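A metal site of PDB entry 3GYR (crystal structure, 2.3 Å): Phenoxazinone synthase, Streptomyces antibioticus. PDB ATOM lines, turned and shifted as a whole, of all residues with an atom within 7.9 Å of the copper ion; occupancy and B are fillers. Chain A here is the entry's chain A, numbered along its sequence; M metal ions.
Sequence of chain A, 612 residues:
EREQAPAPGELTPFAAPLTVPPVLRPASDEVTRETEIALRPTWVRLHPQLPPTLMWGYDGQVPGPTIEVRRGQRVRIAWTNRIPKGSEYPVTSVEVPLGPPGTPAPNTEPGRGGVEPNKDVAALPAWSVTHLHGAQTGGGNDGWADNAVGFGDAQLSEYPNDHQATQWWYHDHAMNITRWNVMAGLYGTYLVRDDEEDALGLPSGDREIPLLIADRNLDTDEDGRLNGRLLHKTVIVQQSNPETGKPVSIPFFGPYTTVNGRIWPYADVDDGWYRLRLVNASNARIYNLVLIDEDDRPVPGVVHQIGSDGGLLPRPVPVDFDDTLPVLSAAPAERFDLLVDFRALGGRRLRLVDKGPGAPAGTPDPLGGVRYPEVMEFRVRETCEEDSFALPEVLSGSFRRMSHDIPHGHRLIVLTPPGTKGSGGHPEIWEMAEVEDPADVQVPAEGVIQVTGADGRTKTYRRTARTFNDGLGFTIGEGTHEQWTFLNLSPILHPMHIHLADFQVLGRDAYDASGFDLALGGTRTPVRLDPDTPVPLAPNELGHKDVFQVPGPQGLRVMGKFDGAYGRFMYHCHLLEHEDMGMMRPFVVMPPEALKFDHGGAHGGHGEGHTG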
ATOM      1  N   HIS A 404      14.917  -6.087 -24.403  1.00  0.00           N
ATOM      2  CA  HIS A 404      14.281  -4.881 -23.856  1.00  0.00           C
ATOM      3  C   HIS A 404      15.120  -3.612 -24.095  1.00  0.00           C
ATOM      4  O   HIS A 404      14.623  -2.510 -23.908  1.00  0.00           O
ATOM      5  CB  HIS A 404      13.985  -5.049 -22.366  1.00  0.00           C
ATOM      6  CG  HIS A 404      13.088  -3.986 -21.811  1.00  0.00           C
ATOM      7  ND1 HIS A 404      13.513  -3.047 -20.903  1.00  0.00           N
ATOM      8  CD2 HIS A 404      11.790  -3.686 -22.069  1.00  0.00           C
ATOM      9  CE1 HIS A 404      12.525  -2.229 -20.605  1.00  0.00           C
ATOM     10  NE2 HIS A 404      11.464  -2.600 -21.298  1.00  0.00           N
ATOM     11  N   ASP A 405      16.379  -3.769 -24.541  1.00  0.00           N
ATOM     12  CA  ASP A 405      17.262  -2.635 -24.864  1.00  0.00           C
ATOM     13  C   ASP A 405      16.914  -1.934 -26.148  1.00  0.00           C
ATOM     14  O   ASP A 405      17.361  -0.811 -26.371  1.00  0.00           O
ATOM     15  CB  ASP A 405      18.709  -3.106 -25.047  1.00  0.00           C
ATOM     16  CG  ASP A 405      19.439  -3.284 -23.740  1.00  0.00           C
ATOM     17  OD1 ASP A 405      18.807  -3.191 -22.655  1.00  0.00           O
ATOM     18  OD2 ASP A 405      20.654  -3.553 -23.796  1.00  0.00           O
ATOM     19  N   ILE A 406      16.215  -2.634 -27.039  1.00  0.00           N
ATOM     20  CA  ILE A 406      15.827  -1.987 -28.280  1.00  0.00           C
ATOM     21  C   ILE A 406      14.794  -0.924 -27.920  1.00  0.00           C
ATOM     22  O   ILE A 406      13.878  -1.174 -27.136  1.00  0.00           O
ATOM     23  CB  ILE A 406      15.342  -3.006 -29.330  1.00  0.00           C
ATOM     24  CG1 ILE A 406      15.416  -2.417 -30.760  1.00  0.00           C
ATOM     25  CG2 ILE A 406      13.958  -3.495 -29.001  1.00  0.00           C
ATOM     26  CD1 ILE A 406      15.990  -3.411 -31.852  1.00  0.00           C
ATOM     27  N   PRO A 407      14.994   0.287 -28.434  1.00  0.00           N
ATOM     28  CA  PRO A 407      13.998   1.336 -28.128  1.00  0.00           C
ATOM     29  C   PRO A 407      12.580   0.861 -28.510  1.00  0.00           C
ATOM     30  O   PRO A 407      12.404   0.250 -29.567  1.00  0.00           O
ATOM     31  CB  PRO A 407      14.422   2.511 -29.028  1.00  0.00           C
ATOM     32  CG  PRO A 407      15.839   2.150 -29.523  1.00  0.00           C
ATOM     33  CD  PRO A 407      15.908   0.671 -29.525  1.00  0.00           C
ATOM     34  N   HIS A 408      11.600   1.138 -27.667  1.00  0.00           N
ATOM     35  CA  HIS A 408      10.233   0.669 -27.954  1.00  0.00           C
ATOM     36  C   HIS A 408       9.180   1.538 -27.294  1.00  0.00           C
ATOM     37  O   HIS A 408       9.487   2.285 -26.379  1.00  0.00           O
ATOM     38  CB  HIS A 408      10.062  -0.768 -27.450  1.00  0.00           C
ATOM     39  CG  HIS A 408      10.373  -0.941 -25.991  1.00  0.00           C
ATOM     40  ND1 HIS A 408      11.659  -1.143 -25.519  1.00  0.00           N
ATOM     41  CD2 HIS A 408       9.561  -0.959 -24.903  1.00  0.00           C
ATOM     42  CE1 HIS A 408      11.624  -1.276 -24.206  1.00  0.00           C
ATOM     43  NE2 HIS A 408      10.373  -1.160 -23.803  1.00  0.00           N
ATOM     44  N   GLY A 409       7.946   1.400 -27.733  1.00  0.00           N
ATOM     45  CA  GLY A 409       6.809   2.007 -27.055  1.00  0.00           C
ATOM     46  C   GLY A 409       6.152   0.972 -26.150  1.00  0.00           C
ATOM     47  O   GLY A 409       6.585  -0.183 -26.104  1.00  0.00           O
ATOM     48  N   HIS A 410       5.094   1.386 -25.437  1.00  0.00           N
ATOM     49  CA  HIS A 410       4.512   0.612 -24.353  1.00  0.00           C
ATOM     50  C   HIS A 410       2.977   0.676 -24.390  1.00  0.00           C
ATOM     51  O   HIS A 410       2.393   1.750 -24.492  1.00  0.00           O
ATOM     52  CB  HIS A 410       5.003   1.161 -23.011  1.00  0.00           C
ATOM     53  CG  HIS A 410       6.432   0.846 -22.718  1.00  0.00           C
ATOM     54  ND1 HIS A 410       7.452   1.756 -22.914  1.00  0.00           N
ATOM     55  CD2 HIS A 410       7.021  -0.251 -22.173  1.00  0.00           C
ATOM     56  CE1 HIS A 410       8.598   1.237 -22.517  1.00  0.00           C
ATOM     57  NE2 HIS A 410       8.370   0.001 -22.095  1.00  0.00           N
ATOM     58  N   GLU A 482       7.207  -2.508 -29.885  1.00  0.00           N
ATOM     59  CA  GLU A 482       6.396  -2.100 -28.746  1.00  0.00           C
ATOM     60  C   GLU A 482       6.366  -3.252 -27.772  1.00  0.00           C
ATOM     61  O   GLU A 482       6.295  -4.410 -28.206  1.00  0.00           O
ATOM     62  CB  GLU A 482       4.970  -1.761 -29.165  1.00  0.00           C
ATOM     63  CG  GLU A 482       4.790  -0.448 -29.902  1.00  0.00           C
ATOM     64  CD  GLU A 482       3.315   0.022 -29.922  1.00  0.00           C
ATOM     65  OE1 GLU A 482       2.421  -0.657 -29.361  1.00  0.00           O
ATOM     66  OE2 GLU A 482       3.053   1.078 -30.529  1.00  0.00           O
ATOM     67  N   GLN A 483       6.413  -2.922 -26.477  1.00  0.00           N
ATOM     68  CA  GLN A 483       6.147  -3.870 -25.406  1.00  0.00           C
ATOM     69  C   GLN A 483       4.716  -3.724 -24.962  1.00  0.00           C
ATOM     70  O   GLN A 483       4.254  -2.637 -24.578  1.00  0.00           O
ATOM     71  CB  GLN A 483       7.033  -3.647 -24.180  1.00  0.00           C
ATOM     72  CG  GLN A 483       6.732  -4.653 -23.036  1.00  0.00           C
ATOM     73  CD  GLN A 483       7.679  -4.467 -21.816  1.00  0.00           C
ATOM     74  OE1 GLN A 483       7.341  -3.783 -20.845  1.00  0.00           O
ATOM     75  NE2 GLN A 483       8.859  -5.031 -21.884  1.00  0.00           N
ATOM     76  N   TRP A 484       4.010  -4.846 -24.992  1.00  0.00           N
ATOM     77  CA  TRP A 484       2.653  -4.869 -24.548  1.00  0.00           C
ATOM     78  C   TRP A 484       2.578  -5.620 -23.239  1.00  0.00           C
ATOM     79  O   TRP A 484       3.143  -6.706 -23.129  1.00  0.00           O
ATOM     80  CB  TRP A 484       1.797  -5.556 -25.589  1.00  0.00           C
ATOM     81  CG  TRP A 484       1.555  -4.725 -26.803  1.00  0.00           C
ATOM     82  CD1 TRP A 484       2.369  -3.757 -27.333  1.00  0.00           C
ATOM     83  CD2 TRP A 484       0.412  -4.819 -27.659  1.00  0.00           C
ATOM     84  NE1 TRP A 484       1.797  -3.242 -28.492  1.00  0.00           N
ATOM     85  CE2 TRP A 484       0.594  -3.870 -28.695  1.00  0.00           C
ATOM     86  CE3 TRP A 484      -0.739  -5.609 -27.650  1.00  0.00           C
ATOM     87  CZ2 TRP A 484      -0.341  -3.701 -29.722  1.00  0.00           C
ATOM     88  CZ3 TRP A 484      -1.669  -5.447 -28.688  1.00  0.00           C
ATOM     89  CH2 TRP A 484      -1.473  -4.488 -29.698  1.00  0.00           C
ATOM     90  N   THR A 485       1.909  -5.040 -22.251  1.00  0.00           N
ATOM     91  CA  THR A 485       1.679  -5.742 -21.008  1.00  0.00           C
ATOM     92  C   THR A 485       0.199  -6.109 -20.947  1.00  0.00           C
ATOM     93  O   THR A 485      -0.651  -5.263 -21.125  1.00  0.00           O
ATOM     94  CB  THR A 485       2.051  -4.880 -19.779  1.00  0.00           C
ATOM     95  OG1 THR A 485       3.426  -4.550 -19.815  1.00  0.00           O
ATOM     96  CG2 THR A 485       1.764  -5.657 -18.478  1.00  0.00           C
ATOM     97  N   LEU A 506       8.659 -11.705 -22.651  1.00  0.00           N
ATOM     98  CA  LEU A 506       9.745 -11.101 -21.869  1.00  0.00           C
ATOM     99  C   LEU A 506       9.689 -11.503 -20.395  1.00  0.00           C
ATOM    100  O   LEU A 506      10.741 -11.675 -19.790  1.00  0.00           O
ATOM    101  CB  LEU A 506       9.786  -9.568 -22.011  1.00  0.00           C
ATOM    102  CG  LEU A 506      10.222  -9.008 -23.375  1.00  0.00           C
ATOM    103  CD1 LEU A 506      10.499  -7.534 -23.213  1.00  0.00           C
ATOM    104  CD2 LEU A 506      11.419  -9.750 -24.001  1.00  0.00           C
ATOM    105  N   ARG A 557       4.394  -9.746 -20.107  1.00  0.00           N
ATOM    106  CA  ARG A 557       5.132  -8.780 -20.912  1.00  0.00           C
ATOM    107  C   ARG A 557       5.590  -9.410 -22.225  1.00  0.00           C
ATOM    108  O   ARG A 557       6.420 -10.324 -22.224  1.00  0.00           O
ATOM    109  CB  ARG A 557       6.333  -8.223 -20.117  1.00  0.00           C
ATOM    110  CG  ARG A 557       5.958  -7.127 -19.119  1.00  0.00           C
ATOM    111  CD  ARG A 557       7.121  -6.643 -18.235  1.00  0.00           C
ATOM    112  NE  ARG A 557       7.494  -7.640 -17.235  1.00  0.00           N
ATOM    113  CZ  ARG A 557       8.682  -8.263 -17.212  1.00  0.00           C
ATOM    114  NH1 ARG A 557       9.612  -7.963 -18.108  1.00  0.00           N
ATOM    115  NH2 ARG A 557       8.921  -9.177 -16.290  1.00  0.00           N
ATOM    116  N   MET A 559       7.072  -8.520 -26.312  1.00  0.00           N
ATOM    117  CA  MET A 559       7.610  -7.480 -27.163  1.00  0.00           C
ATOM    118  C   MET A 559       7.619  -7.904 -28.615  1.00  0.00           C
ATOM    119  O   MET A 559       7.886  -9.078 -28.920  1.00  0.00           O
ATOM    120  CB  MET A 559       9.029  -7.114 -26.759  1.00  0.00           C
ATOM    121  CG  MET A 559       9.469  -5.807 -27.374  1.00  0.00           C
ATOM    122  SD  MET A 559      11.113  -5.366 -26.880  1.00  0.00           S
ATOM    123  CE  MET A 559      10.824  -4.914 -25.192  1.00  0.00           C
HETATM  124 CU    CU M   1       9.922  -1.161 -21.734  1.00  0.00          CU
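A ring nitrogen (ND1) of His 408 sits at hydrogen-bond distance from the backbone carbonyl oxygen of Ile 406 (2.7 Å).
O of Gly 409 is in hydrogen-bond range of N of Gln 483 (2.8 Å).
Gln 483 touches the copper ion (OE1 to CU, 3.8 Å).
The copper ion is bound by a ring nitrogen (NE2) of His 410 (2.0 Å), a ring nitrogen (NE2) of His 408 (2.1 Å) and a ring nitrogen (NE2) of His 404 (2.2 Å).
The copper ion has three donor atoms within binding distance.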
